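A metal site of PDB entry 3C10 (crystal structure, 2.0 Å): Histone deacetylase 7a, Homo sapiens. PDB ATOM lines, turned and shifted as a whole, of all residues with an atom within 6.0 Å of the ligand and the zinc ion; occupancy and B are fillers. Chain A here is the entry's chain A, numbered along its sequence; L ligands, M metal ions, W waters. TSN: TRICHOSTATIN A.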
ATOM      1  N   SER A  59     -24.003  19.547  14.715  1.00  0.00           N
ATOM      2  CA  SER A  59     -24.501  18.172  14.593  1.00  0.00           C
ATOM      3  C   SER A  59     -25.889  18.118  13.970  1.00  0.00           C
ATOM      4  O   SER A  59     -26.137  17.312  13.071  1.00  0.00           O
ATOM      5  CB  SER A  59     -24.469  17.445  15.954  1.00  0.00           C
ATOM      6  OG  SER A  59     -25.552  16.557  16.122  1.00  0.00           O
ATOM      7  N   ARG A  60     -26.793  18.980  14.444  1.00  0.00           N
ATOM      8  CA  ARG A  60     -28.163  18.974  13.917  1.00  0.00           C
ATOM      9  C   ARG A  60     -28.418  20.000  12.800  1.00  0.00           C
ATOM     10  O   ARG A  60     -29.570  20.186  12.392  1.00  0.00           O
ATOM     11  CB  ARG A  60     -29.189  19.125  15.052  1.00  0.00           C
ATOM     12  CG  ARG A  60     -28.871  20.157  16.105  1.00  0.00           C
ATOM     13  CD  ARG A  60     -29.914  20.096  17.219  1.00  0.00           C
ATOM     14  NE  ARG A  60     -29.560  20.948  18.359  1.00  0.00           N
ATOM     15  CZ  ARG A  60     -29.194  20.523  19.559  1.00  0.00           C
ATOM     16  NH1 ARG A  60     -29.116  19.224  19.838  1.00  0.00           N
ATOM     17  NH2 ARG A  60     -28.901  21.403  20.510  1.00  0.00           N
ATOM     18  N   HIS A  61     -27.350  20.637  12.327  1.00  0.00           N
ATOM     19  CA  HIS A  61     -27.404  21.697  11.315  1.00  0.00           C
ATOM     20  C   HIS A  61     -26.319  21.504  10.245  1.00  0.00           C
ATOM     21  O   HIS A  61     -25.269  22.129  10.331  1.00  0.00           O
ATOM     22  CB  HIS A  61     -27.258  23.087  11.963  1.00  0.00           C
ATOM     23  CG  HIS A  61     -28.256  23.367  13.048  1.00  0.00           C
ATOM     24  ND1 HIS A  61     -29.620  23.363  12.828  1.00  0.00           N
ATOM     25  CD2 HIS A  61     -28.090  23.702  14.352  1.00  0.00           C
ATOM     26  CE1 HIS A  61     -30.251  23.642  13.955  1.00  0.00           C
ATOM     27  NE2 HIS A  61     -29.343  23.855  14.892  1.00  0.00           N
ATOM     28  N   PRO A  62     -26.573  20.645   9.243  1.00  0.00           N
ATOM     29  CA  PRO A  62     -25.587  20.301   8.236  1.00  0.00           C
ATOM     30  C   PRO A  62     -25.089  21.449   7.354  1.00  0.00           C
ATOM     31  O   PRO A  62     -23.945  21.399   6.869  1.00  0.00           O
ATOM     32  CB  PRO A  62     -26.302  19.238   7.397  1.00  0.00           C
ATOM     33  CG  PRO A  62     -27.737  19.371   7.727  1.00  0.00           C
ATOM     34  CD  PRO A  62     -27.835  19.924   9.046  1.00  0.00           C
ATOM     35  N   ASP A 146     -35.316  22.901   9.066  1.00  0.00           N
ATOM     36  CA  ASP A 146     -33.955  22.856   8.518  1.00  0.00           C
ATOM     37  C   ASP A 146     -33.315  24.226   8.491  1.00  0.00           C
ATOM     38  O   ASP A 146     -32.113  24.367   8.715  1.00  0.00           O
ATOM     39  CB  ASP A 146     -34.003  22.343   7.064  1.00  0.00           C
ATOM     40  CG  ASP A 146     -34.629  20.957   6.941  1.00  0.00           C
ATOM     41  OD1 ASP A 146     -34.290  20.078   7.761  1.00  0.00           O
ATOM     42  OD2 ASP A 146     -35.458  20.779   6.010  1.00  0.00           O
ATOM     43  N   PRO A 187     -26.822  28.632   0.968  1.00  0.00           N
ATOM     44  CA  PRO A 187     -27.087  28.367  -0.427  1.00  0.00           C
ATOM     45  C   PRO A 187     -28.334  29.114  -0.888  1.00  0.00           C
ATOM     46  O   PRO A 187     -28.960  29.824  -0.055  1.00  0.00           O
ATOM     47  CB  PRO A 187     -27.282  26.839  -0.458  1.00  0.00           C
ATOM     48  CG  PRO A 187     -27.827  26.535   0.906  1.00  0.00           C
ATOM     49  CD  PRO A 187     -27.134  27.485   1.824  1.00  0.00           C
ATOM     50  N   HIS A 189     -30.581  28.021  -4.116  1.00  0.00           N
ATOM     51  CA  HIS A 189     -31.413  27.512  -5.212  1.00  0.00           C
ATOM     52  C   HIS A 189     -32.842  27.092  -4.848  1.00  0.00           C
ATOM     53  O   HIS A 189     -33.681  27.020  -5.735  1.00  0.00           O
ATOM     54  CB  HIS A 189     -30.656  26.507  -6.130  1.00  0.00           C
ATOM     55  CG  HIS A 189     -30.497  25.132  -5.571  1.00  0.00           C
ATOM     56  ND1 HIS A 189     -30.595  24.004  -6.364  1.00  0.00           N
ATOM     57  CD2 HIS A 189     -30.212  24.686  -4.319  1.00  0.00           C
ATOM     58  CE1 HIS A 189     -30.378  22.938  -5.624  1.00  0.00           C
ATOM     59  NE2 HIS A 189     -30.155  23.318  -4.383  1.00  0.00           N
ATOM     60  N   HIS A 190     -33.136  26.898  -3.558  1.00  0.00           N
ATOM     61  CA  HIS A 190     -34.503  26.591  -3.138  1.00  0.00           C
ATOM     62  C   HIS A 190     -35.369  27.823  -2.809  1.00  0.00           C
ATOM     63  O   HIS A 190     -36.546  27.688  -2.630  1.00  0.00           O
ATOM     64  CB  HIS A 190     -34.471  25.661  -1.891  1.00  0.00           C
ATOM     65  CG  HIS A 190     -33.821  24.330  -2.153  1.00  0.00           C
ATOM     66  ND1 HIS A 190     -34.242  23.511  -3.168  1.00  0.00           N
ATOM     67  CD2 HIS A 190     -32.806  23.689  -1.524  1.00  0.00           C
ATOM     68  CE1 HIS A 190     -33.543  22.379  -3.135  1.00  0.00           C
ATOM     69  NE2 HIS A 190     -32.627  22.486  -2.189  1.00  0.00           N
ATOM     70  N   GLY A 198     -35.305  25.008   2.682  1.00  0.00           N
ATOM     71  CA  GLY A 198     -34.148  24.167   2.265  1.00  0.00           C
ATOM     72  C   GLY A 198     -32.763  24.801   2.447  1.00  0.00           C
ATOM     73  O   GLY A 198     -31.879  24.650   1.578  1.00  0.00           O
ATOM     74  N   PHE A 199     -32.580  25.502   3.561  1.00  0.00           N
ATOM     75  CA  PHE A 199     -31.318  26.177   3.887  1.00  0.00           C
ATOM     76  C   PHE A 199     -31.105  27.550   3.224  1.00  0.00           C
ATOM     77  O   PHE A 199     -30.137  28.228   3.553  1.00  0.00           O
ATOM     78  CB  PHE A 199     -30.068  25.296   3.688  1.00  0.00           C
ATOM     79  CG  PHE A 199     -30.099  23.973   4.458  1.00  0.00           C
ATOM     80  CD1 PHE A 199     -30.696  23.877   5.693  1.00  0.00           C
ATOM     81  CD2 PHE A 199     -29.486  22.834   3.917  1.00  0.00           C
ATOM     82  CE1 PHE A 199     -30.707  22.631   6.404  1.00  0.00           C
ATOM     83  CE2 PHE A 199     -29.481  21.575   4.635  1.00  0.00           C
ATOM     84  CZ  PHE A 199     -30.126  21.502   5.874  1.00  0.00           C
ATOM     85  N   CYS A 200     -32.030  27.957   2.349  1.00  0.00           N
ATOM     86  CA  CYS A 200     -31.873  29.063   1.409  1.00  0.00           C
ATOM     87  C   CYS A 200     -32.813  30.202   1.707  1.00  0.00           C
ATOM     88  O   CYS A 200     -33.993  29.987   2.044  1.00  0.00           O
ATOM     89  CB  CYS A 200     -32.151  28.609  -0.043  1.00  0.00           C
ATOM     90  SG  CYS A 200     -31.210  27.207  -0.681  1.00  0.00           S
ATOM     91  N   ASP A 227     -26.350  20.340  -8.178  1.00  0.00           N
ATOM     92  CA  ASP A 227     -26.773  19.953  -6.863  1.00  0.00           C
ATOM     93  C   ASP A 227     -27.745  18.732  -7.026  1.00  0.00           C
ATOM     94  O   ASP A 227     -28.513  18.695  -7.961  1.00  0.00           O
ATOM     95  CB  ASP A 227     -27.489  21.115  -6.189  1.00  0.00           C
ATOM     96  CG  ASP A 227     -27.689  20.883  -4.722  1.00  0.00           C
ATOM     97  OD1 ASP A 227     -28.633  20.173  -4.342  1.00  0.00           O
ATOM     98  OD2 ASP A 227     -26.940  21.431  -3.886  1.00  0.00           O
ATOM     99  N   VAL A 228     -27.670  17.750  -6.115  1.00  0.00           N
ATOM    100  CA  VAL A 228     -28.527  16.567  -6.160  1.00  0.00           C
ATOM    101  C   VAL A 228     -30.022  16.883  -5.986  1.00  0.00           C
ATOM    102  O   VAL A 228     -30.880  16.074  -6.353  1.00  0.00           O
ATOM    103  CB  VAL A 228     -28.042  15.499  -5.112  1.00  0.00           C
ATOM    104  CG1 VAL A 228     -28.583  15.781  -3.672  1.00  0.00           C
ATOM    105  CG2 VAL A 228     -28.446  14.072  -5.602  1.00  0.00           C
ATOM    106  N   HIS A 229     -30.348  18.070  -5.420  1.00  0.00           N
ATOM    107  CA  HIS A 229     -31.766  18.501  -5.251  1.00  0.00           C
ATOM    108  C   HIS A 229     -32.183  19.374  -6.391  1.00  0.00           C
ATOM    109  O   HIS A 229     -31.348  20.132  -6.922  1.00  0.00           O
ATOM    110  CB  HIS A 229     -31.965  19.307  -3.957  1.00  0.00           C
ATOM    111  CG  HIS A 229     -31.540  18.552  -2.752  1.00  0.00           C
ATOM    112  ND1 HIS A 229     -30.304  18.712  -2.156  1.00  0.00           N
ATOM    113  CD2 HIS A 229     -32.190  17.600  -2.026  1.00  0.00           C
ATOM    114  CE1 HIS A 229     -30.205  17.873  -1.141  1.00  0.00           C
ATOM    115  NE2 HIS A 229     -31.334  17.191  -1.048  1.00  0.00           N
ATOM    116  N   PHE A 258     -36.543  15.423  -1.642  1.00  0.00           N
ATOM    117  CA  PHE A 258     -36.645  16.853  -1.349  1.00  0.00           C
ATOM    118  C   PHE A 258     -36.150  17.627  -2.596  1.00  0.00           C
ATOM    119  O   PHE A 258     -35.132  17.289  -3.145  1.00  0.00           O
ATOM    120  CB  PHE A 258     -35.820  17.235  -0.115  1.00  0.00           C
ATOM    121  CG  PHE A 258     -35.920  18.685   0.225  1.00  0.00           C
ATOM    122  CD1 PHE A 258     -35.000  19.611  -0.303  1.00  0.00           C
ATOM    123  CD2 PHE A 258     -36.967  19.160   1.037  1.00  0.00           C
ATOM    124  CE1 PHE A 258     -35.106  21.005   0.019  1.00  0.00           C
ATOM    125  CE2 PHE A 258     -37.091  20.532   1.330  1.00  0.00           C
ATOM    126  CZ  PHE A 258     -36.150  21.464   0.805  1.00  0.00           C
ATOM    127  N   GLY A 319     -23.761  22.546  -6.320  1.00  0.00           N
ATOM    128  CA  GLY A 319     -23.890  21.854  -5.042  1.00  0.00           C
ATOM    129  C   GLY A 319     -23.045  20.609  -5.214  1.00  0.00           C
ATOM    130  O   GLY A 319     -22.836  20.160  -6.307  1.00  0.00           O
ATOM    131  N   ASP A 321     -23.615  17.710  -3.202  1.00  0.00           N
ATOM    132  CA  ASP A 321     -24.295  16.659  -2.477  1.00  0.00           C
ATOM    133  C   ASP A 321     -24.624  15.365  -3.240  1.00  0.00           C
ATOM    134  O   ASP A 321     -25.126  14.422  -2.635  1.00  0.00           O
ATOM    135  CB  ASP A 321     -25.539  17.174  -1.768  1.00  0.00           C
ATOM    136  CG  ASP A 321     -26.343  18.205  -2.585  1.00  0.00           C
ATOM    137  OD1 ASP A 321     -26.088  18.483  -3.779  1.00  0.00           O
ATOM    138  OD2 ASP A 321     -27.277  18.709  -1.948  1.00  0.00           O
ATOM    139  N   PRO A 329     -30.491   9.725   2.788  1.00  0.00           N
ATOM    140  CA  PRO A 329     -31.437  10.844   2.889  1.00  0.00           C
ATOM    141  C   PRO A 329     -30.906  12.198   2.411  1.00  0.00           C
ATOM    142  O   PRO A 329     -31.701  13.058   2.084  1.00  0.00           O
ATOM    143  CB  PRO A 329     -31.750  10.894   4.405  1.00  0.00           C
ATOM    144  CG  PRO A 329     -30.547  10.325   5.052  1.00  0.00           C
ATOM    145  CD  PRO A 329     -30.151   9.190   4.128  1.00  0.00           C
ATOM    146  N   LEU A 330     -29.594  12.376   2.353  1.00  0.00           N
ATOM    147  CA  LEU A 330     -28.984  13.640   1.946  1.00  0.00           C
ATOM    148  C   LEU A 330     -28.414  13.657   0.506  1.00  0.00           C
ATOM    149  O   LEU A 330     -27.859  14.665   0.073  1.00  0.00           O
ATOM    150  CB  LEU A 330     -27.858  14.021   2.946  1.00  0.00           C
ATOM    151  CG  LEU A 330     -28.335  14.630   4.269  1.00  0.00           C
ATOM    152  CD1 LEU A 330     -27.247  14.552   5.341  1.00  0.00           C
ATOM    153  CD2 LEU A 330     -28.845  16.090   4.123  1.00  0.00           C
ATOM    154  N   GLU A 360     -23.678  25.603  -3.653  1.00  0.00           N
ATOM    155  CA  GLU A 360     -25.016  25.404  -3.183  1.00  0.00           C
ATOM    156  C   GLU A 360     -24.911  24.443  -2.040  1.00  0.00           C
ATOM    157  O   GLU A 360     -24.359  24.815  -0.984  1.00  0.00           O
ATOM    158  CB  GLU A 360     -25.944  24.902  -4.310  1.00  0.00           C
ATOM    159  CG  GLU A 360     -26.055  25.914  -5.468  1.00  0.00           C
ATOM    160  CD  GLU A 360     -27.085  27.063  -5.182  1.00  0.00           C
ATOM    161  OE1 GLU A 360     -27.371  27.864  -6.108  1.00  0.00           O
ATOM    162  OE2 GLU A 360     -27.601  27.174  -4.060  1.00  0.00           O
ATOM    163  N   GLY A 361     -25.401  23.229  -2.234  1.00  0.00           N
ATOM    164  CA  GLY A 361     -25.449  22.248  -1.169  1.00  0.00           C
ATOM    165  C   GLY A 361     -24.220  21.364  -1.118  1.00  0.00           C
ATOM    166  O   GLY A 361     -23.255  21.592  -1.797  1.00  0.00           O
ATOM    167  N   GLY A 362     -24.257  20.325  -0.309  1.00  0.00           N
ATOM    168  CA  GLY A 362     -23.077  19.460  -0.178  1.00  0.00           C
ATOM    169  C   GLY A 362     -22.479  19.772   1.188  1.00  0.00           C
ATOM    170  O   GLY A 362     -22.118  20.934   1.476  1.00  0.00           O
ATOM    171  N   HIS A 363     -22.349  18.759   2.023  1.00  0.00           N
ATOM    172  CA  HIS A 363     -21.840  18.986   3.383  1.00  0.00           C
ATOM    173  C   HIS A 363     -20.721  18.054   3.910  1.00  0.00           C
ATOM    174  O   HIS A 363     -20.193  18.303   5.004  1.00  0.00           O
ATOM    175  CB  HIS A 363     -22.998  19.075   4.370  1.00  0.00           C
ATOM    176  CG  HIS A 363     -23.386  17.766   4.981  1.00  0.00           C
ATOM    177  ND1 HIS A 363     -22.597  17.110   5.906  1.00  0.00           N
ATOM    178  CD2 HIS A 363     -24.496  17.003   4.815  1.00  0.00           C
ATOM    179  CE1 HIS A 363     -23.190  15.992   6.276  1.00  0.00           C
ATOM    180  NE2 HIS A 363     -24.347  15.907   5.634  1.00  0.00           N
HETATM  181  O1  TSN L   1     -29.924  21.771  -2.098  1.00  0.00           O
HETATM  182  O2  TSN L   1     -28.600  20.353   0.130  1.00  0.00           O
HETATM  183  O3  TSN L   1     -33.024  15.613   3.886  1.00  0.00           O
HETATM  184  N1  TSN L   1     -29.520  22.114  -0.812  1.00  0.00           N
HETATM  185  N2  TSN L   1     -29.768  15.556   9.428  1.00  0.00           N
HETATM  186  C1  TSN L   1     -31.969  16.334   5.887  1.00  0.00           C
HETATM  187  C2  TSN L   1     -31.451  15.055   6.145  1.00  0.00           C
HETATM  188  C3  TSN L   1     -30.724  14.816   7.314  1.00  0.00           C
HETATM  189  C4  TSN L   1     -30.508  15.829   8.257  1.00  0.00           C
HETATM  190  C5  TSN L   1     -31.024  17.118   7.997  1.00  0.00           C
HETATM  191  C6  TSN L   1     -31.746  17.364   6.816  1.00  0.00           C
HETATM  192  C7  TSN L   1     -32.740  16.571   4.604  1.00  0.00           C
HETATM  193  C8  TSN L   1     -33.167  17.940   4.141  1.00  0.00           C
HETATM  194  C9  TSN L   1     -32.140  18.392   3.108  1.00  0.00           C
HETATM  195  C10 TSN L   1     -31.986  19.641   2.625  1.00  0.00           C
HETATM  196  C11 TSN L   1     -30.920  19.857   1.621  1.00  0.00           C
HETATM  197  C12 TSN L   1     -30.593  21.057   1.123  1.00  0.00           C
HETATM  198  C13 TSN L   1     -29.509  21.166   0.130  1.00  0.00           C
HETATM  199  C14 TSN L   1     -34.596  17.871   3.588  1.00  0.00           C
HETATM  200  C15 TSN L   1     -32.882  20.769   3.071  1.00  0.00           C
HETATM  201  C17 TSN L   1     -28.342  15.839   9.501  1.00  0.00           C
HETATM  202  C16 TSN L   1     -30.436  14.942  10.576  1.00  0.00           C
HETATM  203 ZN    ZN M   1     -28.781  19.983  -2.423  1.00  0.00          ZN
HETATM  204  O   HOH W   1     -26.692  20.126   1.829  1.00  0.00           O
HETATM  205  O   HOH W   2     -31.602  20.173   9.583  1.00  0.00           O
HETATM  206  O   HOH W   3     -25.264  16.323  10.801  1.00  0.00           O
HETATM  207  O   HOH W   4     -32.301  15.427   1.107  1.00  0.00           O
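An oxygen (O1) of the ligand lies close to a ring nitrogen (NE2) of His 189. N1 of the ligand sits at hydrogen-bond distance from NE2 of His 190 (3.4 Å).
The side-chain sulfur of Cys 200 sits at hydrogen-bond distance from the backbone carbonyl oxygen of Gly 198 (3.5 Å). The side-chain carboxylate of Asp 227 sits at hydrogen-bond distance from the backbone NH of Gly 361, 2.9 Å away. OD1 of Asp 321 lies within hydrogen-bond range of N of Val 228 (2.9 Å). The side-chain carboxylate (OE2) of Glu 360 sits at hydrogen-bond distance from the backbone NH (N) of His 189. N of His 189 sits at hydrogen-bond distance from SG of Cys 200. OD1 of Asp 227 sits close to NE2 of His 189, at 3.5 Å. N of His 190 is in hydrogen-bond range of SG of Cys 200 (3.5 Å). A ring nitrogen (NE2) of His 189 sits at hydrogen-bond distance from a ring nitrogen (NE2) of His 190 (3.4 Å).
O of Pro 329 lies close to O3 of the ligand, at 3.4 Å. CG of Pro 62 touches C5 of the ligand, 3.99 Å away. Asp 146 touches the ligand. CA of Gly 198 touches C15 of the ligand, at 3.7 Å. Phe 199 touches the ligand. Phe 258 touches the ligand. CD2 of Leu 330 touches C2 of the ligand, 3.5 Å away. Gly 361 touches the ligand (CA to O2, 3.9 Å). Hydrophobic or aromatic side chains within 4 Å of the ligand: Pro 62, His 189, His 190, Phe 199, His 229, Phe 258 and Leu 330. Of the 23 residues printed, 13 come within 4 Å of the ligand.
Within 4 Å of the zinc ion: Asp 227, His 229 and Asp 321. The nearest printed residue that does not touch the zinc ion is His 189 (4.1 Å).
The zinc ion is bound by OD1 of Asp 227, ND1 of His 229, OD2 of Asp 321, O1 of the ligand and O2 of the ligand. The zinc ion has five donor atoms within binding distance. Slightly farther from the zinc ion lies the side-chain carboxylate (OD2) of Asp 227 (2.8 Å).
Water W4 lies within hydrogen-bond range of O of Pro 329 (2.6 Å), O3 of the ligand (2.9 Å) and NE2 of His 229 (2.9 Å). Water W2 lies within hydrogen-bond range of the side-chain carboxylate (OD1) of Asp 146 (3.2 Å) and the backbone carbonyl oxygen (O) of Arg 60 (3.5 Å).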
